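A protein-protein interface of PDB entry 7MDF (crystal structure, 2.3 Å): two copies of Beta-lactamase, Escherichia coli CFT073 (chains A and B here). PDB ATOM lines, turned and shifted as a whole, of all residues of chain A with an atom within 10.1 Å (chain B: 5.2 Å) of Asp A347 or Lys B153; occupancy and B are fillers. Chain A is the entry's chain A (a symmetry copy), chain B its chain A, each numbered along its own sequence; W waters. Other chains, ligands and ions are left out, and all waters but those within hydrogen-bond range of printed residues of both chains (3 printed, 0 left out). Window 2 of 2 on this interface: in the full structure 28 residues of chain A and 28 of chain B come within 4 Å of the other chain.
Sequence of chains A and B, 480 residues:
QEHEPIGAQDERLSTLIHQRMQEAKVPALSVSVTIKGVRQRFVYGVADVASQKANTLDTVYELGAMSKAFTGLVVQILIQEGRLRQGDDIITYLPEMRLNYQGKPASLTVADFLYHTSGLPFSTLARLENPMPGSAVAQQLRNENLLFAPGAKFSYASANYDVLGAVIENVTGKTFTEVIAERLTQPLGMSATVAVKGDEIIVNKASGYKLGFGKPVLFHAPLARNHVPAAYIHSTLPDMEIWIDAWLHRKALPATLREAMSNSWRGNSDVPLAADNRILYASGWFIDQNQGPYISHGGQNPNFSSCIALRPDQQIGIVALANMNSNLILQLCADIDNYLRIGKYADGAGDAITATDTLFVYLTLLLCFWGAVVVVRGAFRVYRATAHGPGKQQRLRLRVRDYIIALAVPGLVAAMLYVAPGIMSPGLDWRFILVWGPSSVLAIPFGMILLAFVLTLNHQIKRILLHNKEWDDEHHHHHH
The backbone carbonyl oxygen (O) of Thr B117 sits at hydrogen-bond distance from the backbone NH (N) of Gly B151. NH2 of Arg A20 is in hydrogen-bond range of O of Ala A346 (2.6 Å). The backbone carbonyl oxygen (O) of Ala A334 is in hydrogen-bond range of the side-chain amide nitrogen (ND2) of Asn A338 (3.3 Å). The guanidinium group (NH2) of Arg A341 sits at hydrogen-bond distance from the side-chain amide oxygen (OD1) of Asn A338 (2.9 Å).
Among the printed residues, merely in contact across the chains: Asn A338 with Pro B272, Ile A342 with Val B271, Ile A342 with Pro B272, Tyr A345 with Pro B272 and Ala A346 with Pro B272.
Water W1 bridges the backbone carbonyl oxygen (O) of Ala B152 and the backbone carbonyl oxygen (O) of Tyr A345. Water W3 bridges the side-chain amino group (NZ) of Lys B153 (2.9 Å) and the side-chain carboxylate (OD1) of Asp A347 (3.1 Å). Water W2 bridges the side-chain amino group (NZ) of Lys B153 and the backbone NH (N) of Asp A347.
No position is printed for both chains.
NZ of Lys A344 sits at hydrogen-bond distance from O of Gly B151, at 3.1 Å. The side-chain amino group (NZ) of Lys B153 lies within salt-bridge range of the side-chain carboxylate (OD1) of Asp A347, at 2.4 Å. NH2 of Arg A341 lies within hydrogen-bond range of O of Val B271 (3.0 Å).
Of the 12 printed residues of chain B, 4 touch a printed residue of chain A. Printed residues of chain B that touch a printed residue of chain A: Gly B151, Lys B153, Val B271 and Pro B272. Hydrophobic or aromatic side chains of chain B within 4 Å of the printed part of chain A: Pro B272. Of the 21 printed residues of chain A, 7 touch a printed residue of chain B. Among the printed residues, 8 pairs touch across the chains. Among the printed residues, Asp or Glu carboxylates within 4 Å of a Lys or Arg side-chain nitrogen of the other chain: Asp A347 with Lys B153.
Of chain A, only Asp A347 (2.4 Å) comes within 4 Å of Lys B153. No residue of chain A comes within 4 Å of Thr B117. No residue of chain A comes within 4 Å of Ala B152. No residue of chain A comes within 4 Å of Ser B155. Of the printed residues of chain A, Pro B272 touches Asn A338, Ile A342, Tyr A345 and Ala A346. Printed residues of chain B within 4 Å of Lys A344: Gly B151 (3.1 Å). Of the printed residues of chain A, Val B271 touches Arg A341 and Ile A342. The nearest residue of chain A that does not touch Lys B153 is Ala A346 (4.5 Å). The nearest printed residue of chain B that does not touch Lys A344 is Pro B272 (4.4 Å).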
ATOM      1  N   LEU A  16     -28.773  33.705  31.888  1.00  0.00           N
ATOM      2  CA  LEU A  16     -27.482  33.077  31.616  1.00  0.00           C
ATOM      3  C   LEU A  16     -26.446  33.435  32.680  1.00  0.00           C
ATOM      4  O   LEU A  16     -25.808  32.555  33.267  1.00  0.00           O
ATOM      5  CB  LEU A  16     -26.992  33.495  30.224  1.00  0.00           C
ATOM      6  CG  LEU A  16     -25.521  33.221  29.855  1.00  0.00           C
ATOM      7  CD1 LEU A  16     -25.164  31.731  29.904  1.00  0.00           C
ATOM      8  CD2 LEU A  16     -25.281  33.786  28.481  1.00  0.00           C
ATOM      9  N   GLN A  19     -27.058  32.055  36.137  1.00  0.00           N
ATOM     10  CA  GLN A  19     -26.781  30.629  36.121  1.00  0.00           C
ATOM     11  C   GLN A  19     -25.285  30.352  36.197  1.00  0.00           C
ATOM     12  O   GLN A  19     -24.837  29.534  37.010  1.00  0.00           O
ATOM     13  CB  GLN A  19     -27.382  29.997  34.867  1.00  0.00           C
ATOM     14  CG  GLN A  19     -27.292  28.504  34.882  1.00  0.00           C
ATOM     15  CD  GLN A  19     -27.402  27.909  33.489  1.00  0.00           C
ATOM     16  OE1 GLN A  19     -26.486  27.243  33.019  1.00  0.00           O
ATOM     17  NE2 GLN A  19     -28.529  28.151  32.821  1.00  0.00           N
ATOM     18  N   ARG A  20     -24.491  31.023  35.351  1.00  0.00           N
ATOM     19  CA  ARG A  20     -23.040  30.843  35.397  1.00  0.00           C
ATOM     20  C   ARG A  20     -22.449  31.325  36.717  1.00  0.00           C
ATOM     21  O   ARG A  20     -21.465  30.751  37.196  1.00  0.00           O
ATOM     22  CB  ARG A  20     -22.381  31.567  34.231  1.00  0.00           C
ATOM     23  CG  ARG A  20     -22.652  30.949  32.892  1.00  0.00           C
ATOM     24  CD  ARG A  20     -22.158  29.516  32.819  1.00  0.00           C
ATOM     25  NE  ARG A  20     -22.083  29.114  31.422  1.00  0.00           N
ATOM     26  CZ  ARG A  20     -23.015  28.423  30.789  1.00  0.00           C
ATOM     27  NH1 ARG A  20     -24.052  27.916  31.429  1.00  0.00           N
ATOM     28  NH2 ARG A  20     -22.902  28.234  29.480  1.00  0.00           N
ATOM     29  N   GLU A  23     -23.231  28.447  39.148  1.00  0.00           N
ATOM     30  CA  GLU A  23     -22.372  27.300  38.867  1.00  0.00           C
ATOM     31  C   GLU A  23     -20.927  27.594  39.236  1.00  0.00           C
ATOM     32  O   GLU A  23     -20.225  26.726  39.762  1.00  0.00           O
ATOM     33  CB  GLU A  23     -22.452  26.907  37.392  1.00  0.00           C
ATOM     34  CG  GLU A  23     -23.787  26.414  36.945  1.00  0.00           C
ATOM     35  CD  GLU A  23     -23.956  26.526  35.444  1.00  0.00           C
ATOM     36  OE1 GLU A  23     -23.178  27.280  34.813  1.00  0.00           O
ATOM     37  OE2 GLU A  23     -24.871  25.869  34.902  1.00  0.00           O
ATOM     38  N   ASN A 327     -13.215  28.951  35.770  1.00  0.00           N
ATOM     39  CA  ASN A 327     -13.329  28.731  34.328  1.00  0.00           C
ATOM     40  C   ASN A 327     -14.696  29.151  33.793  1.00  0.00           C
ATOM     41  O   ASN A 327     -14.808  29.559  32.629  1.00  0.00           O
ATOM     42  CB  ASN A 327     -13.061  27.254  34.007  1.00  0.00           C
ATOM     43  CG  ASN A 327     -12.848  26.994  32.514  1.00  0.00           C
ATOM     44  OD1 ASN A 327     -12.217  27.788  31.810  1.00  0.00           O
ATOM     45  ND2 ASN A 327     -13.397  25.880  32.026  1.00  0.00           N
ATOM     46  N   LEU A 328     -15.745  29.084  34.621  1.00  0.00           N
ATOM     47  CA  LEU A 328     -17.056  29.542  34.164  1.00  0.00           C
ATOM     48  C   LEU A 328     -17.075  31.044  33.919  1.00  0.00           C
ATOM     49  O   LEU A 328     -17.862  31.514  33.097  1.00  0.00           O
ATOM     50  CB  LEU A 328     -18.136  29.130  35.164  1.00  0.00           C
ATOM     51  CG  LEU A 328     -18.284  27.593  35.209  1.00  0.00           C
ATOM     52  CD1 LEU A 328     -18.932  27.124  36.457  1.00  0.00           C
ATOM     53  CD2 LEU A 328     -19.094  27.119  34.057  1.00  0.00           C
ATOM     54  N   GLN A 331     -15.000  31.559  30.531  1.00  0.00           N
ATOM     55  CA  GLN A 331     -15.756  31.228  29.331  1.00  0.00           C
ATOM     56  C   GLN A 331     -17.009  32.070  29.144  1.00  0.00           C
ATOM     57  O   GLN A 331     -17.598  32.016  28.056  1.00  0.00           O
ATOM     58  CB  GLN A 331     -16.160  29.752  29.348  1.00  0.00           C
ATOM     59  CG  GLN A 331     -14.979  28.803  29.582  1.00  0.00           C
ATOM     60  CD  GLN A 331     -13.805  29.077  28.637  1.00  0.00           C
ATOM     61  OE1 GLN A 331     -13.991  29.292  27.435  1.00  0.00           O
ATOM     62  NE2 GLN A 331     -12.595  29.090  29.186  1.00  0.00           N
ATOM     63  N   LEU A 332     -17.417  32.844  30.164  1.00  0.00           N
ATOM     64  CA  LEU A 332     -18.709  33.540  30.130  1.00  0.00           C
ATOM     65  C   LEU A 332     -18.801  34.534  28.979  1.00  0.00           C
ATOM     66  O   LEU A 332     -19.873  34.694  28.384  1.00  0.00           O
ATOM     67  CB  LEU A 332     -18.950  34.261  31.456  1.00  0.00           C
ATOM     68  CG  LEU A 332     -20.135  35.231  31.554  1.00  0.00           C
ATOM     69  CD1 LEU A 332     -21.461  34.503  31.349  1.00  0.00           C
ATOM     70  CD2 LEU A 332     -20.097  35.922  32.893  1.00  0.00           C
ATOM     71  N   ALA A 334     -17.515  34.251  25.974  1.00  0.00           N
ATOM     72  CA  ALA A 334     -17.885  33.467  24.791  1.00  0.00           C
ATOM     73  C   ALA A 334     -19.349  33.027  24.836  1.00  0.00           C
ATOM     74  O   ALA A 334     -20.052  33.097  23.822  1.00  0.00           O
ATOM     75  CB  ALA A 334     -16.972  32.248  24.651  1.00  0.00           C
ATOM     76  N   ASP A 335     -19.815  32.539  25.995  1.00  0.00           N
ATOM     77  CA  ASP A 335     -21.243  32.259  26.187  1.00  0.00           C
ATOM     78  C   ASP A 335     -22.108  33.455  25.791  1.00  0.00           C
ATOM     79  O   ASP A 335     -23.081  33.318  25.039  1.00  0.00           O
ATOM     80  CB  ASP A 335     -21.522  31.905  27.647  1.00  0.00           C
ATOM     81  CG  ASP A 335     -20.977  30.565  28.040  1.00  0.00           C
ATOM     82  OD1 ASP A 335     -20.899  29.680  27.167  1.00  0.00           O
ATOM     83  OD2 ASP A 335     -20.641  30.394  29.233  1.00  0.00           O
ATOM     84  N   ASN A 338     -22.057  33.940  22.058  1.00  0.00           N
ATOM     85  CA  ASN A 338     -22.989  33.009  21.413  1.00  0.00           C
ATOM     86  C   ASN A 338     -24.407  33.521  21.539  1.00  0.00           C
ATOM     87  O   ASN A 338     -25.177  33.502  20.568  1.00  0.00           O
ATOM     88  CB  ASN A 338     -22.901  31.607  22.027  1.00  0.00           C
ATOM     89  CG  ASN A 338     -21.599  30.898  21.701  1.00  0.00           C
ATOM     90  OD1 ASN A 338     -21.084  30.998  20.576  1.00  0.00           O
ATOM     91  ND2 ASN A 338     -21.070  30.152  22.676  1.00  0.00           N
ATOM     92  N   ARG A 341     -25.074  36.349  19.286  1.00  0.00           N
ATOM     93  CA  ARG A 341     -24.910  35.986  17.890  1.00  0.00           C
ATOM     94  C   ARG A 341     -26.079  35.132  17.398  1.00  0.00           C
ATOM     95  O   ARG A 341     -26.704  35.455  16.381  1.00  0.00           O
ATOM     96  CB  ARG A 341     -23.565  35.277  17.701  1.00  0.00           C
ATOM     97  CG  ARG A 341     -23.155  35.029  16.249  1.00  0.00           C
ATOM     98  CD  ARG A 341     -21.728  34.422  16.139  1.00  0.00           C
ATOM     99  NE  ARG A 341     -21.518  33.291  17.037  1.00  0.00           N
ATOM    100  CZ  ARG A 341     -21.887  32.034  16.801  1.00  0.00           C
ATOM    101  NH1 ARG A 341     -22.411  31.661  15.637  1.00  0.00           N
ATOM    102  NH2 ARG A 341     -21.727  31.121  17.760  1.00  0.00           N
ATOM    103  N   ILE A 342     -26.421  34.058  18.115  1.00  0.00           N
ATOM    104  CA  ILE A 342     -27.430  33.111  17.642  1.00  0.00           C
ATOM    105  C   ILE A 342     -28.543  32.858  18.651  1.00  0.00           C
ATOM    106  O   ILE A 342     -29.435  32.058  18.376  1.00  0.00           O
ATOM    107  CB  ILE A 342     -26.785  31.771  17.222  1.00  0.00           C
ATOM    108  CG1 ILE A 342     -25.991  31.175  18.387  1.00  0.00           C
ATOM    109  CG2 ILE A 342     -25.818  31.965  16.059  1.00  0.00           C
ATOM    110  CD1 ILE A 342     -25.442  29.812  18.101  1.00  0.00           C
ATOM    111  N   LYS A 344     -28.352  31.263  21.505  1.00  0.00           N
ATOM    112  CA  LYS A 344     -28.191  30.052  22.302  1.00  0.00           C
ATOM    113  C   LYS A 344     -26.765  29.971  22.817  1.00  0.00           C
ATOM    114  O   LYS A 344     -25.903  30.772  22.458  1.00  0.00           O
ATOM    115  CB  LYS A 344     -28.560  28.775  21.528  1.00  0.00           C
ATOM    116  CG  LYS A 344     -28.260  28.757  20.056  1.00  0.00           C
ATOM    117  CD  LYS A 344     -28.847  27.483  19.434  1.00  0.00           C
ATOM    118  CE  LYS A 344     -29.345  27.710  18.018  1.00  0.00           C
ATOM    119  NZ  LYS A 344     -29.497  26.445  17.257  1.00  0.00           N
ATOM    120  N   TYR A 345     -26.529  29.001  23.694  1.00  0.00           N
ATOM    121  CA  TYR A 345     -25.239  28.849  24.349  1.00  0.00           C
ATOM    122  C   TYR A 345     -25.168  27.446  24.926  1.00  0.00           C
ATOM    123  O   TYR A 345     -26.117  26.685  24.782  1.00  0.00           O
ATOM    124  CB  TYR A 345     -25.022  29.912  25.446  1.00  0.00           C
ATOM    125  CG  TYR A 345     -26.191  30.082  26.438  1.00  0.00           C
ATOM    126  CD1 TYR A 345     -26.372  29.194  27.493  1.00  0.00           C
ATOM    127  CD2 TYR A 345     -27.093  31.138  26.323  1.00  0.00           C
ATOM    128  CE1 TYR A 345     -27.390  29.348  28.395  1.00  0.00           C
ATOM    129  CE2 TYR A 345     -28.134  31.299  27.232  1.00  0.00           C
ATOM    130  CZ  TYR A 345     -28.274  30.400  28.262  1.00  0.00           C
ATOM    131  OH  TYR A 345     -29.308  30.528  29.168  1.00  0.00           O
ATOM    132  N   ALA A 346     -23.952  26.935  25.026  1.00  0.00           N
ATOM    133  CA  ALA A 346     -23.714  25.578  25.478  1.00  0.00           C
ATOM    134  C   ALA A 346     -23.701  25.530  27.002  1.00  0.00           C
ATOM    135  O   ALA A 346     -23.756  26.555  27.680  1.00  0.00           O
ATOM    136  CB  ALA A 346     -22.400  25.053  24.905  1.00  0.00           C
ATOM    137  N   ASP A 347     -23.630  24.320  27.545  1.00  0.00           N
ATOM    138  CA  ASP A 347     -23.631  24.168  28.990  1.00  0.00           C
ATOM    139  C   ASP A 347     -22.316  24.679  29.585  1.00  0.00           C
ATOM    140  O   ASP A 347     -21.304  24.859  28.887  1.00  0.00           O
ATOM    141  CB  ASP A 347     -23.854  22.706  29.383  1.00  0.00           C
ATOM    142  CG  ASP A 347     -25.191  22.162  28.902  1.00  0.00           C
ATOM    143  OD1 ASP A 347     -25.260  21.652  27.761  1.00  0.00           O
ATOM    144  OD2 ASP A 347     -26.180  22.251  29.664  1.00  0.00           O
ATOM    145  N   GLY A 348     -22.346  24.919  30.901  1.00  0.00           N
ATOM    146  CA  GLY A 348     -21.164  25.311  31.644  1.00  0.00           C
ATOM    147  C   GLY A 348     -20.006  24.348  31.451  1.00  0.00           C
ATOM    148  O   GLY A 348     -20.154  23.128  31.608  1.00  0.00           O
ATOM    149  N   ALA A 349     -18.849  24.890  31.082  1.00  0.00           N
ATOM    150  CA  ALA A 349     -17.632  24.098  30.984  1.00  0.00           C
ATOM    151  C   ALA A 349     -17.193  23.612  32.371  1.00  0.00           C
ATOM    152  O   ALA A 349     -17.736  24.015  33.405  1.00  0.00           O
ATOM    153  CB  ALA A 349     -16.527  24.915  30.313  1.00  0.00           C
ATOM    154  N   GLY A 350     -16.212  22.702  32.389  1.00  0.00           N
ATOM    155  CA  GLY A 350     -15.677  22.225  33.650  1.00  0.00           C
ATOM    156  C   GLY A 350     -14.740  23.241  34.279  1.00  0.00           C
ATOM    157  O   GLY A 350     -14.418  24.273  33.691  1.00  0.00           O
ATOM    158  N   ASP A 351     -14.287  22.932  35.492  1.00  0.00           N
ATOM    159  CA  ASP A 351     -13.427  23.843  36.247  1.00  0.00           C
ATOM    160  C   ASP A 351     -12.388  23.033  37.011  1.00  0.00           C
ATOM    161  O   ASP A 351     -12.747  22.170  37.823  1.00  0.00           O
ATOM    162  CB  ASP A 351     -14.262  24.712  37.198  1.00  0.00           C
ATOM    163  CG  ASP A 351     -13.428  25.745  37.935  1.00  0.00           C
ATOM    164  OD1 ASP A 351     -12.885  26.663  37.271  1.00  0.00           O
ATOM    165  OD2 ASP A 351     -13.327  25.641  39.179  1.00  0.00           O
ATOM    166  N   HIS B 116     -23.304  17.526  12.432  1.00  0.00           N
ATOM    167  CA  HIS B 116     -23.091  16.939  13.760  1.00  0.00           C
ATOM    168  C   HIS B 116     -23.771  17.761  14.859  1.00  0.00           C
ATOM    169  O   HIS B 116     -23.146  18.122  15.861  1.00  0.00           O
ATOM    170  CB  HIS B 116     -21.592  16.787  14.082  1.00  0.00           C
ATOM    171  CG  HIS B 116     -20.816  15.970  13.091  1.00  0.00           C
ATOM    172  ND1 HIS B 116     -20.576  14.623  13.264  1.00  0.00           N
ATOM    173  CD2 HIS B 116     -20.186  16.319  11.940  1.00  0.00           C
ATOM    174  CE1 HIS B 116     -19.860  14.171  12.245  1.00  0.00           C
ATOM    175  NE2 HIS B 116     -19.605  15.181  11.432  1.00  0.00           N
ATOM    176  N   THR B 117     -25.059  18.075  14.662  1.00  0.00           N
ATOM    177  CA  THR B 117     -25.887  18.735  15.675  1.00  0.00           C
ATOM    178  C   THR B 117     -27.091  17.868  16.024  1.00  0.00           C
ATOM    179  O   THR B 117     -28.201  18.371  16.275  1.00  0.00           O
ATOM    180  CB  THR B 117     -26.343  20.115  15.216  1.00  0.00           C
ATOM    181  OG1 THR B 117     -27.187  19.983  14.066  1.00  0.00           O
ATOM    182  CG2 THR B 117     -25.153  20.968  14.827  1.00  0.00           C
ATOM    183  N   SER B 118     -26.868  16.545  16.063  1.00  0.00           N
ATOM    184  CA  SER B 118     -27.933  15.563  16.222  1.00  0.00           C
ATOM    185  C   SER B 118     -28.118  15.084  17.652  1.00  0.00           C
ATOM    186  O   SER B 118     -29.241  14.780  18.045  1.00  0.00           O
ATOM    187  CB  SER B 118     -27.675  14.352  15.318  1.00  0.00           C
ATOM    188  OG  SER B 118     -26.705  13.477  15.882  1.00  0.00           O
ATOM    189  N   PHE B 148     -28.625  16.088  23.686  1.00  0.00           N
ATOM    190  CA  PHE B 148     -29.046  17.479  23.720  1.00  0.00           C
ATOM    191  C   PHE B 148     -30.059  17.657  22.598  1.00  0.00           C
ATOM    192  O   PHE B 148     -30.192  16.802  21.722  1.00  0.00           O
ATOM    193  CB  PHE B 148     -27.858  18.450  23.567  1.00  0.00           C
ATOM    194  CG  PHE B 148     -26.993  18.160  22.370  1.00  0.00           C
ATOM    195  CD1 PHE B 148     -27.363  18.591  21.101  1.00  0.00           C
ATOM    196  CD2 PHE B 148     -25.812  17.428  22.505  1.00  0.00           C
ATOM    197  CE1 PHE B 148     -26.565  18.304  19.994  1.00  0.00           C
ATOM    198  CE2 PHE B 148     -25.022  17.142  21.400  1.00  0.00           C
ATOM    199  CZ  PHE B 148     -25.394  17.589  20.153  1.00  0.00           C
ATOM    200  N   ALA B 149     -30.781  18.761  22.644  1.00  0.00           N
ATOM    201  CA  ALA B 149     -31.818  18.996  21.653  1.00  0.00           C
ATOM    202  C   ALA B 149     -31.182  19.152  20.280  1.00  0.00           C
ATOM    203  O   ALA B 149     -30.202  19.886  20.146  1.00  0.00           O
ATOM    204  CB  ALA B 149     -32.638  20.238  22.011  1.00  0.00           C
ATOM    205  N   GLY B 151     -29.738  20.329  16.910  1.00  0.00           N
ATOM    206  CA  GLY B 151     -29.347  21.661  16.521  1.00  0.00           C
ATOM    207  C   GLY B 151     -28.723  22.506  17.611  1.00  0.00           C
ATOM    208  O   GLY B 151     -28.271  23.615  17.314  1.00  0.00           O
ATOM    209  N   ALA B 152     -28.683  22.031  18.864  1.00  0.00           N
ATOM    210  CA  ALA B 152     -28.311  22.911  19.969  1.00  0.00           C
ATOM    211  C   ALA B 152     -26.801  23.065  20.121  1.00  0.00           C
ATOM    212  O   ALA B 152     -26.356  24.054  20.710  1.00  0.00           O
ATOM    213  CB  ALA B 152     -28.899  22.422  21.293  1.00  0.00           C
ATOM    214  N   LYS B 153     -26.004  22.110  19.634  1.00  0.00           N
ATOM    215  CA  LYS B 153     -24.563  22.305  19.612  1.00  0.00           C
ATOM    216  C   LYS B 153     -23.901  21.363  18.621  1.00  0.00           C
ATOM    217  O   LYS B 153     -24.495  20.379  18.168  1.00  0.00           O
ATOM    218  CB  LYS B 153     -23.925  22.134  21.001  1.00  0.00           C
ATOM    219  CG  LYS B 153     -24.205  20.849  21.763  1.00  0.00           C
ATOM    220  CD  LYS B 153     -23.881  21.130  23.240  1.00  0.00           C
ATOM    221  CE  LYS B 153     -24.459  20.121  24.221  1.00  0.00           C
ATOM    222  NZ  LYS B 153     -24.886  20.785  25.504  1.00  0.00           N
ATOM    223  N   PHE B 154     -22.648  21.706  18.288  1.00  0.00           N
ATOM    224  CA  PHE B 154     -21.762  20.840  17.523  1.00  0.00           C
ATOM    225  C   PHE B 154     -21.194  19.774  18.438  1.00  0.00           C
ATOM    226  O   PHE B 154     -20.684  20.087  19.510  1.00  0.00           O
ATOM    227  CB  PHE B 154     -20.611  21.623  16.905  1.00  0.00           C
ATOM    228  CG  PHE B 154     -19.591  20.744  16.259  1.00  0.00           C
ATOM    229  CD1 PHE B 154     -19.793  20.276  14.952  1.00  0.00           C
ATOM    230  CD2 PHE B 154     -18.448  20.339  16.955  1.00  0.00           C
ATOM    231  CE1 PHE B 154     -18.864  19.439  14.330  1.00  0.00           C
ATOM    232  CE2 PHE B 154     -17.521  19.486  16.349  1.00  0.00           C
ATOM    233  CZ  PHE B 154     -17.732  19.035  15.024  1.00  0.00           C
ATOM    234  N   SER B 155     -21.300  18.512  18.023  1.00  0.00           N
ATOM    235  CA  SER B 155     -20.775  17.402  18.819  1.00  0.00           C
ATOM    236  C   SER B 155     -20.474  16.270  17.835  1.00  0.00           C
ATOM    237  O   SER B 155     -21.395  15.595  17.381  1.00  0.00           O
ATOM    238  CB  SER B 155     -21.759  16.970  19.899  1.00  0.00           C
ATOM    239  OG  SER B 155     -21.203  15.944  20.705  1.00  0.00           O
ATOM    240  N   VAL B 271     -24.450  27.179  15.819  1.00  0.00           N
ATOM    241  CA  VAL B 271     -24.150  26.424  17.037  1.00  0.00           C
ATOM    242  C   VAL B 271     -23.317  27.310  17.957  1.00  0.00           C
ATOM    243  O   VAL B 271     -22.628  28.229  17.474  1.00  0.00           O
ATOM    244  CB  VAL B 271     -23.399  25.114  16.738  1.00  0.00           C
ATOM    245  CG1 VAL B 271     -24.352  24.018  16.304  1.00  0.00           C
ATOM    246  CG2 VAL B 271     -22.317  25.345  15.701  1.00  0.00           C
ATOM    247  N   PRO B 272     -23.358  27.088  19.272  1.00  0.00           N
ATOM    248  CA  PRO B 272     -22.425  27.790  20.160  1.00  0.00           C
ATOM    249  C   PRO B 272     -20.982  27.477  19.773  1.00  0.00           C
ATOM    250  O   PRO B 272     -20.649  26.357  19.369  1.00  0.00           O
ATOM    251  CB  PRO B 272     -22.769  27.232  21.546  1.00  0.00           C
ATOM    252  CG  PRO B 272     -24.147  26.706  21.418  1.00  0.00           C
ATOM    253  CD  PRO B 272     -24.243  26.188  20.022  1.00  0.00           C
HETATM  254  O   HOH W   1     -27.710  25.563  22.687  1.00  0.00           O
HETATM  255  O   HOH W   2     -21.899  21.726  26.071  1.00  0.00           O
HETATM  256  O   HOH W   3     -27.232  22.519  25.485  1.00  0.00           O
